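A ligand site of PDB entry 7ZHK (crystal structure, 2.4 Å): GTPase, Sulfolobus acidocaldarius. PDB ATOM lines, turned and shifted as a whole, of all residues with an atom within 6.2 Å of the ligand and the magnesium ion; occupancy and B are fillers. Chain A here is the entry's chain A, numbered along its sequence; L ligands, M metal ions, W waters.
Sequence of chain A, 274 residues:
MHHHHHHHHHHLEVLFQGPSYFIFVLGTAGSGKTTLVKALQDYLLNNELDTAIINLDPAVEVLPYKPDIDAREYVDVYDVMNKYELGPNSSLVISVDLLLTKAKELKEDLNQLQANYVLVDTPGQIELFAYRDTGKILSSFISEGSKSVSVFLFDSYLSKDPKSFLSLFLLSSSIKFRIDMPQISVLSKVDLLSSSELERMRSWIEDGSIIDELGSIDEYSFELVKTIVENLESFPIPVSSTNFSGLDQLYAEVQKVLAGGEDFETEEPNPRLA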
ATOM      1  N   GLY A  27       6.454  25.540   9.461  1.00  0.00           N
ATOM      2  CA  GLY A  27       6.541  25.110  10.844  1.00  0.00           C
ATOM      3  C   GLY A  27       7.685  24.140  11.030  1.00  0.00           C
ATOM      4  O   GLY A  27       8.244  23.610  10.071  1.00  0.00           O
ATOM      5  N   THR A  28       8.023  23.908  12.292  1.00  0.00           N
ATOM      6  CA  THR A  28       9.077  22.959  12.620  1.00  0.00           C
ATOM      7  C   THR A  28       8.687  21.555  12.184  1.00  0.00           C
ATOM      8  O   THR A  28       7.524  21.249  11.899  1.00  0.00           O
ATOM      9  CB  THR A  28       9.370  22.979  14.125  1.00  0.00           C
ATOM     10  OG1 THR A  28       8.164  22.713  14.848  1.00  0.00           O
ATOM     11  CG2 THR A  28       9.923  24.340  14.537  1.00  0.00           C
ATOM     12  N   ALA A  29       9.696  20.678  12.124  1.00  0.00           N
ATOM     13  CA  ALA A  29       9.471  19.296  11.730  1.00  0.00           C
ATOM     14  C   ALA A  29       8.518  18.613  12.703  1.00  0.00           C
ATOM     15  O   ALA A  29       8.674  18.715  13.927  1.00  0.00           O
ATOM     16  CB  ALA A  29      10.785  18.538  11.668  1.00  0.00           C
ATOM     17  N   GLY A  30       7.511  17.921  12.168  1.00  0.00           N
ATOM     18  CA  GLY A  30       6.546  17.236  12.991  1.00  0.00           C
ATOM     19  C   GLY A  30       5.545  18.122  13.684  1.00  0.00           C
ATOM     20  O   GLY A  30       4.785  17.634  14.520  1.00  0.00           O
ATOM     21  N   SER A  31       5.509  19.417  13.361  1.00  0.00           N
ATOM     22  CA  SER A  31       4.550  20.317  13.969  1.00  0.00           C
ATOM     23  C   SER A  31       3.145  20.175  13.397  1.00  0.00           C
ATOM     24  O   SER A  31       2.206  20.763  13.945  1.00  0.00           O
ATOM     25  CB  SER A  31       5.019  21.768  13.826  1.00  0.00           C
ATOM     26  OG  SER A  31       5.034  22.159  12.459  1.00  0.00           O
ATOM     27  N   GLY A  32       2.967  19.413  12.328  1.00  0.00           N
ATOM     28  CA  GLY A  32       1.670  19.139  11.761  1.00  0.00           C
ATOM     29  C   GLY A  32       1.363  19.784  10.429  1.00  0.00           C
ATOM     30  O   GLY A  32       0.174  19.905  10.088  1.00  0.00           O
ATOM     31  N   LYS A  33       2.377  20.205   9.661  1.00  0.00           N
ATOM     32  CA  LYS A  33       2.124  20.879   8.392  1.00  0.00           C
ATOM     33  C   LYS A  33       1.320  20.011   7.437  1.00  0.00           C
ATOM     34  O   LYS A  33       0.278  20.423   6.923  1.00  0.00           O
ATOM     35  CB  LYS A  33       3.448  21.297   7.745  1.00  0.00           C
ATOM     36  CG  LYS A  33       4.324  22.180   8.623  1.00  0.00           C
ATOM     37  CD  LYS A  33       5.575  22.606   7.859  1.00  0.00           C
ATOM     38  CE  LYS A  33       6.546  21.449   7.714  1.00  0.00           C
ATOM     39  NZ  LYS A  33       7.151  21.048   9.014  1.00  0.00           N
ATOM     40  N   THR A  34       1.806  18.792   7.182  1.00  0.00           N
ATOM     41  CA  THR A  34       1.155  17.937   6.193  1.00  0.00           C
ATOM     42  C   THR A  34      -0.265  17.558   6.612  1.00  0.00           C
ATOM     43  O   THR A  34      -1.183  17.547   5.783  1.00  0.00           O
ATOM     44  CB  THR A  34       2.002  16.683   5.951  1.00  0.00           C
ATOM     45  OG1 THR A  34       3.294  17.068   5.467  1.00  0.00           O
ATOM     46  CG2 THR A  34       1.345  15.802   4.911  1.00  0.00           C
ATOM     47  N   THR A  35      -0.459  17.262   7.899  1.00  0.00           N
ATOM     48  CA  THR A  35      -1.792  16.911   8.375  1.00  0.00           C
ATOM     49  C   THR A  35      -2.736  18.095   8.296  1.00  0.00           C
ATOM     50  O   THR A  35      -3.920  17.934   7.984  1.00  0.00           O
ATOM     51  CB  THR A  35      -1.712  16.365   9.805  1.00  0.00           C
ATOM     52  OG1 THR A  35      -0.778  15.285   9.864  1.00  0.00           O
ATOM     53  CG2 THR A  35      -3.082  15.860  10.250  1.00  0.00           C
ATOM     54  N   LEU A  36      -2.234  19.299   8.577  1.00  0.00           N
ATOM     55  CA  LEU A  36      -3.079  20.489   8.473  1.00  0.00           C
ATOM     56  C   LEU A  36      -3.497  20.758   7.038  1.00  0.00           C
ATOM     57  O   LEU A  36      -4.613  21.225   6.792  1.00  0.00           O
ATOM     58  CB  LEU A  36      -2.357  21.707   9.055  1.00  0.00           C
ATOM     59  CG  LEU A  36      -3.190  22.990   9.084  1.00  0.00           C
ATOM     60  CD1 LEU A  36      -4.375  22.832  10.023  1.00  0.00           C
ATOM     61  CD2 LEU A  36      -2.344  24.183   9.474  1.00  0.00           C
ATOM     62  N   ASP A  57       7.641  18.804  -0.579  1.00  0.00           N
ATOM     63  CA  ASP A  57       8.541  17.937   0.156  1.00  0.00           C
ATOM     64  C   ASP A  57       8.910  16.757  -0.716  1.00  0.00           C
ATOM     65  O   ASP A  57       8.065  15.867  -0.930  1.00  0.00           O
ATOM     66  CB  ASP A  57       7.896  17.464   1.456  1.00  0.00           C
ATOM     67  CG  ASP A  57       8.887  16.805   2.400  1.00  0.00           C
ATOM     68  OD1 ASP A  57      10.036  16.533   1.980  1.00  0.00           O
ATOM     69  OD2 ASP A  57       8.515  16.558   3.568  1.00  0.00           O
ATOM     70  N   VAL A  60       8.898  12.953   1.462  1.00  0.00           N
ATOM     71  CA  VAL A  60       7.819  12.438   2.296  1.00  0.00           C
ATOM     72  C   VAL A  60       7.399  11.067   1.774  1.00  0.00           C
ATOM     73  O   VAL A  60       7.231  10.868   0.571  1.00  0.00           O
ATOM     74  CB  VAL A  60       6.637  13.422   2.327  1.00  0.00           C
ATOM     75  CG1 VAL A  60       6.168  13.764   0.915  1.00  0.00           C
ATOM     76  CG2 VAL A  60       5.489  12.869   3.153  1.00  0.00           C
ATOM     77  N   ASP A 121       2.297  22.517   0.689  1.00  0.00           N
ATOM     78  CA  ASP A 121       2.990  21.794   1.750  1.00  0.00           C
ATOM     79  C   ASP A 121       4.485  21.897   1.526  1.00  0.00           C
ATOM     80  O   ASP A 121       4.985  21.628   0.430  1.00  0.00           O
ATOM     81  CB  ASP A 121       2.550  20.332   1.784  1.00  0.00           C
ATOM     82  CG  ASP A 121       2.840  19.665   3.107  1.00  0.00           C
ATOM     83  OD1 ASP A 121       3.329  20.346   4.032  1.00  0.00           O
ATOM     84  OD2 ASP A 121       2.573  18.450   3.229  1.00  0.00           O
ATOM     85  N   THR A 122       5.205  22.289   2.566  1.00  0.00           N
ATOM     86  CA  THR A 122       6.626  22.567   2.473  1.00  0.00           C
ATOM     87  C   THR A 122       7.446  21.402   3.017  1.00  0.00           C
ATOM     88  O   THR A 122       6.908  20.515   3.674  1.00  0.00           O
ATOM     89  CB  THR A 122       6.957  23.844   3.267  1.00  0.00           C
ATOM     90  OG1 THR A 122       6.482  23.719   4.608  1.00  0.00           O
ATOM     91  CG2 THR A 122       6.300  25.050   2.609  1.00  0.00           C
ATOM     92  N   PRO A 123       8.759  21.359   2.722  1.00  0.00           N
ATOM     93  CA  PRO A 123       9.604  20.286   3.271  1.00  0.00           C
ATOM     94  C   PRO A 123       9.497  20.158   4.785  1.00  0.00           C
ATOM     95  O   PRO A 123       9.116  21.104   5.471  1.00  0.00           O
ATOM     96  CB  PRO A 123      11.014  20.708   2.845  1.00  0.00           C
ATOM     97  CG  PRO A 123      10.795  21.430   1.558  1.00  0.00           C
ATOM     98  CD  PRO A 123       9.473  22.139   1.697  1.00  0.00           C
ATOM     99  N   GLY A 124       9.840  18.973   5.298  1.00  0.00           N
ATOM    100  CA  GLY A 124       9.651  18.705   6.715  1.00  0.00           C
ATOM    101  C   GLY A 124      10.385  19.686   7.604  1.00  0.00           C
ATOM    102  O   GLY A 124       9.808  20.250   8.547  1.00  0.00           O
ATOM    103  N   LEU A 153       3.234  27.081  12.034  1.00  0.00           N
ATOM    104  CA  LEU A 153       2.670  26.211  13.058  1.00  0.00           C
ATOM    105  C   LEU A 153       3.523  26.265  14.321  1.00  0.00           C
ATOM    106  O   LEU A 153       4.728  25.956  14.280  1.00  0.00           O
ATOM    107  CB  LEU A 153       2.559  24.777  12.552  1.00  0.00           C
ATOM    108  CG  LEU A 153       1.748  24.558  11.280  1.00  0.00           C
ATOM    109  CD1 LEU A 153       1.383  23.102  11.149  1.00  0.00           C
ATOM    110  CD2 LEU A 153       0.507  25.425  11.277  1.00  0.00           C
ATOM    111  N   SER A 188      -0.676  24.546  16.616  1.00  0.00           N
ATOM    112  CA  SER A 188      -1.091  23.271  16.056  1.00  0.00           C
ATOM    113  C   SER A 188      -1.025  22.175  17.125  1.00  0.00           C
ATOM    114  O   SER A 188      -0.398  22.331  18.170  1.00  0.00           O
ATOM    115  CB  SER A 188      -0.191  22.894  14.880  1.00  0.00           C
ATOM    116  OG  SER A 188       1.127  22.621  15.308  1.00  0.00           O
ATOM    117  N   LYS A 189      -1.702  21.058  16.825  1.00  0.00           N
ATOM    118  CA  LYS A 189      -1.733  19.900  17.726  1.00  0.00           C
ATOM    119  C   LYS A 189      -2.273  20.290  19.102  1.00  0.00           C
ATOM    120  O   LYS A 189      -1.790  19.823  20.133  1.00  0.00           O
ATOM    121  CB  LYS A 189      -0.339  19.276  17.849  1.00  0.00           C
ATOM    122  CG  LYS A 189       0.383  19.115  16.523  1.00  0.00           C
ATOM    123  CD  LYS A 189       1.746  18.460  16.692  1.00  0.00           C
ATOM    124  CE  LYS A 189       1.680  16.952  16.692  1.00  0.00           C
ATOM    125  NZ  LYS A 189       3.034  16.352  16.573  1.00  0.00           N
ATOM    126  N   VAL A 190      -3.290  21.162  19.115  1.00  0.00           N
ATOM    127  CA  VAL A 190      -3.812  21.695  20.363  1.00  0.00           C
ATOM    128  C   VAL A 190      -4.609  20.684  21.161  1.00  0.00           C
ATOM    129  O   VAL A 190      -4.942  20.941  22.326  1.00  0.00           O
ATOM    130  CB  VAL A 190      -4.668  22.960  20.094  1.00  0.00           C
ATOM    131  CG1 VAL A 190      -6.089  22.578  19.740  1.00  0.00           C
ATOM    132  CG2 VAL A 190      -4.624  23.903  21.285  1.00  0.00           C
ATOM    133  N   ASP A 191      -4.918  19.522  20.574  1.00  0.00           N
ATOM    134  CA  ASP A 191      -5.572  18.467  21.342  1.00  0.00           C
ATOM    135  C   ASP A 191      -4.636  17.844  22.371  1.00  0.00           C
ATOM    136  O   ASP A 191      -5.101  17.179  23.297  1.00  0.00           O
ATOM    137  CB  ASP A 191      -6.101  17.385  20.401  1.00  0.00           C
ATOM    138  CG  ASP A 191      -5.045  16.863  19.443  1.00  0.00           C
ATOM    139  OD1 ASP A 191      -4.570  17.652  18.610  1.00  0.00           O
ATOM    140  OD2 ASP A 191      -4.685  15.671  19.542  1.00  0.00           O
ATOM    141  N   LEU A 192      -3.327  18.060  22.240  1.00  0.00           N
ATOM    142  CA  LEU A 192      -2.360  17.613  23.238  1.00  0.00           C
ATOM    143  C   LEU A 192      -2.370  18.468  24.489  1.00  0.00           C
ATOM    144  O   LEU A 192      -1.646  18.161  25.444  1.00  0.00           O
ATOM    145  CB  LEU A 192      -0.948  17.611  22.641  1.00  0.00           C
ATOM    146  CG  LEU A 192      -0.700  16.766  21.387  1.00  0.00           C
ATOM    147  CD1 LEU A 192       0.655  17.084  20.794  1.00  0.00           C
ATOM    148  CD2 LEU A 192      -0.813  15.284  21.717  1.00  0.00           C
ATOM    149  N   VAL A 239      -5.473  25.425  16.665  1.00  0.00           N
ATOM    150  CA  VAL A 239      -6.040  24.509  15.683  1.00  0.00           C
ATOM    151  C   VAL A 239      -5.629  23.090  16.053  1.00  0.00           C
ATOM    152  O   VAL A 239      -4.532  22.865  16.564  1.00  0.00           O
ATOM    153  CB  VAL A 239      -5.562  24.859  14.254  1.00  0.00           C
ATOM    154  CG1 VAL A 239      -6.207  23.943  13.214  1.00  0.00           C
ATOM    155  CG2 VAL A 239      -5.864  26.320  13.931  1.00  0.00           C
ATOM    156  N   SER A 240      -6.523  22.138  15.803  1.00  0.00           N
ATOM    157  CA  SER A 240      -6.244  20.717  15.968  1.00  0.00           C
ATOM    158  C   SER A 240      -6.763  19.982  14.738  1.00  0.00           C
ATOM    159  O   SER A 240      -7.983  19.884  14.550  1.00  0.00           O
ATOM    160  CB  SER A 240      -6.869  20.163  17.245  1.00  0.00           C
ATOM    161  OG  SER A 240      -6.902  18.746  17.223  1.00  0.00           O
ATOM    162  N   SER A 241      -5.847  19.478  13.910  1.00  0.00           N
ATOM    163  CA  SER A 241      -6.269  18.782  12.695  1.00  0.00           C
ATOM    164  C   SER A 241      -7.001  17.481  13.024  1.00  0.00           C
ATOM    165  O   SER A 241      -7.937  17.106  12.323  1.00  0.00           O
ATOM    166  CB  SER A 241      -5.057  18.505  11.807  1.00  0.00           C
ATOM    167  OG  SER A 241      -4.437  19.712  11.413  1.00  0.00           O
ATOM    168  N   THR A 242      -6.582  16.797  14.096  1.00  0.00           N
ATOM    169  CA  THR A 242      -7.218  15.528  14.448  1.00  0.00           C
ATOM    170  C   THR A 242      -8.607  15.749  15.036  1.00  0.00           C
ATOM    171  O   THR A 242      -9.522  14.954  14.794  1.00  0.00           O
ATOM    172  CB  THR A 242      -6.343  14.742  15.418  1.00  0.00           C
ATOM    173  OG1 THR A 242      -6.087  15.529  16.579  1.00  0.00           O
ATOM    174  CG2 THR A 242      -5.020  14.369  14.753  1.00  0.00           C
ATOM    175  N   ASN A 243      -8.789  16.822  15.807  1.00  0.00           N
ATOM    176  CA  ASN A 243     -10.122  17.189  16.278  1.00  0.00           C
ATOM    177  C   ASN A 243     -10.897  18.016  15.273  1.00  0.00           C
ATOM    178  O   ASN A 243     -12.101  18.236  15.477  1.00  0.00           O
ATOM    179  CB  ASN A 243     -10.033  17.947  17.603  1.00  0.00           C
ATOM    180  CG  ASN A 243      -9.787  17.030  18.784  1.00  0.00           C
ATOM    181  OD1 ASN A 243      -9.857  15.815  18.672  1.00  0.00           O
ATOM    182  ND2 ASN A 243      -9.489  17.625  19.939  1.00  0.00           N
HETATM  183  P1  LIG L   1       4.972  17.838   9.421  1.00  0.00           P
HETATM  184  O1  LIG L   1       4.335  17.692   8.064  1.00  0.00           O
HETATM  185  O2  LIG L   1       6.368  17.264   9.414  1.00  0.00           O
HETATM  186  O3  LIG L   1       5.058  19.299   9.785  1.00  0.00           O
HETATM  187  O4  LIG L   1       4.098  17.085  10.540  1.00  0.00           O
HETATM  188  P2  LIG L   1       3.027  15.939  10.166  1.00  0.00           P
HETATM  189  O5  LIG L   1       3.656  14.866   9.310  1.00  0.00           O
HETATM  190  O6  LIG L   1       1.801  16.516   9.497  1.00  0.00           O
HETATM  191  O7  LIG L   1       2.665  15.374  11.625  1.00  0.00           O
HETATM  192  C1  LIG L   1       3.687  14.749  12.406  1.00  0.00           C
HETATM  193  C2  LIG L   1       3.018  13.895  13.472  1.00  0.00           C
HETATM  194  O8  LIG L   1       2.128  14.711  14.225  1.00  0.00           O
HETATM  195  C3  LIG L   1       2.197  12.802  12.814  1.00  0.00           C
HETATM  196  O9  LIG L   1       2.532  11.540  13.406  1.00  0.00           O
HETATM  197  C4  LIG L   1       0.754  13.142  13.119  1.00  0.00           C
HETATM  198  O10 LIG L   1       0.012  11.970  13.461  1.00  0.00           O
HETATM  199  C5  LIG L   1       0.832  14.105  14.295  1.00  0.00           C
HETATM  200  N1  LIG L   1      -0.220  15.145  14.216  1.00  0.00           N
HETATM  201  C6  LIG L   1      -0.443  15.980  13.197  1.00  0.00           C
HETATM  202  N2  LIG L   1      -1.475  16.815  13.467  1.00  0.00           N
HETATM  203  C7  LIG L   1      -1.924  16.509  14.701  1.00  0.00           C
HETATM  204  C8  LIG L   1      -2.995  17.004  15.606  1.00  0.00           C
HETATM  205  O11 LIG L   1      -3.754  17.936  15.263  1.00  0.00           O
HETATM  206  N3  LIG L   1      -3.120  16.408  16.801  1.00  0.00           N
HETATM  207  C9  LIG L   1      -2.320  15.405  17.198  1.00  0.00           C
HETATM  208  N4  LIG L   1      -2.519  14.868  18.427  1.00  0.00           N
HETATM  209  N5  LIG L   1      -1.324  14.907  16.421  1.00  0.00           N
HETATM  210  C10 LIG L   1      -1.092  15.416  15.189  1.00  0.00           C
HETATM  211 MG    MG M   1       5.107  16.970   6.262  1.00  0.00          MG
HETATM  212  O   HOH W   1       5.880  16.229   4.418  1.00  0.00           O
HETATM  213  O   HOH W   2      -1.442  10.504  15.944  1.00  0.00           O
HETATM  214  O   HOH W   3       6.996  14.735  10.212  1.00  0.00           O
HETATM  215  O   HOH W   4       4.739  14.971   6.935  1.00  0.00           O
HETATM  216  O   HOH W   5      -0.798  12.194  19.151  1.00  0.00           O
HETATM  217  O   HOH W   6      -3.080  20.432  14.402  1.00  0.00           O
HETATM  218  O   HOH W   7       5.442  18.940   5.597  1.00  0.00           O
HETATM  219  O   HOH W   8       6.993  16.891   7.089  1.00  0.00           O
HETATM  220  O   HOH W   9      -1.841  19.324  12.155  1.00  0.00           O
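An oxygen (O6) of the ligand is in hydrogen-bond range of the backbone NH (N) of Thr 35 (2.9 Å).
O11 of the ligand lies within hydrogen-bond range of N of Ser 241 (2.9 Å).
O3 of the ligand is in hydrogen-bond range of N of Lys 33.
N of Thr 242 sits at hydrogen-bond distance from O11 of the ligand (3.3 Å).
The side-chain hydroxyl (OG1) of Thr 242 sits at hydrogen-bond distance from a nitrogen (N3) of the ligand (3.1 Å).
The side-chain amino group of Lys 189 lies within hydrogen-bond range of an oxygen (O8) of the ligand, 3.0 Å away.
The side-chain amino group of Lys 33 lies within salt-bridge range of an oxygen (O3) of the ligand (2.8 Å).
A nitrogen (N4) of the ligand sits at hydrogen-bond distance from the side-chain carboxylate (OD2) of Asp 191 (2.6 Å).
The backbone NH (N) of Gly 30 is in hydrogen-bond range of an oxygen (O2) of the ligand, at 3.1 Å.
OG1 of Thr 35 is in hydrogen-bond range of O6 of the ligand, at 2.9 Å.
An oxygen (O4) of the ligand is in hydrogen-bond range of the backbone NH (N) of Gly 32 (3.1 Å).
The backbone NH of Thr 34 is in hydrogen-bond range of an oxygen (O6) of the ligand, 3.2 Å away.
OG of Ser 240 is in hydrogen-bond range of N of Asn 243, at 3.0 Å.
OG1 of Thr 242 is in hydrogen-bond range of OG of Ser 240 (3.4 Å).
NZ of Lys 189 is in hydrogen-bond range of O of Gly 30 (3.0 Å).
NZ of Lys 33 lies within hydrogen-bond range of O of Gly 27 (3.0 Å).
The backbone NH (N) of Lys 189 is in hydrogen-bond range of the backbone carbonyl oxygen (O) of Val 239, at 3.4 Å.
The side-chain hydroxyl (OG1) of Thr 34 sits close to the side-chain carboxylate (OD2) of Asp 121, at 2.7 Å.
The backbone carbonyl oxygen of Thr 28 lies within hydrogen-bond range of the side-chain amino group of Lys 33, at 2.9 Å.
The side-chain carboxylate of Asp 191 sits at hydrogen-bond distance from the side-chain hydroxyl of Thr 242 (3.3 Å).
Residues that only touch the ligand: Thr 28 (3.8 Å), Ser 31 (3.6 Å), Leu 192 (3.7 Å) and Ser 240 (3.7 Å).
Hydrophobic or aromatic side chains that line the ligand: Leu 192.
13 residues have an atom within 4 Å of the ligand: Thr 28, Gly 30, Ser 31, Gly 32, Lys 33, Thr 34, Thr 35, Lys 189, Asp 191, Leu 192, Ser 240, Ser 241 and Thr 242.
Of the 27 residues printed, 1 comes within 4 Å of the magnesium ion.
The nearest printed residue that does not touch the magnesium ion is Asp 121 (4.2 Å).
The magnesium ion is bound by OG1 of Thr 34, water W8, O1 of the ligand, water W7, water W1 and water W4.
Water W7 lies within hydrogen-bond range of O of Thr 122 (2.9 Å) and OD1 of Asp 121 (3.0 Å).
Water W6 lies within hydrogen-bond range of O11 of the ligand (2.7 Å), N of Lys 189 (2.9 Å) and N of Ser 241 (3.0 Å).
Water W9 lies within hydrogen-bond range of the side-chain hydroxyl (OG) of Ser 241 (2.7 Å), a nitrogen (N2) of the ligand (2.9 Å) and the backbone carbonyl oxygen (O) of Gly 32 (2.9 Å).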
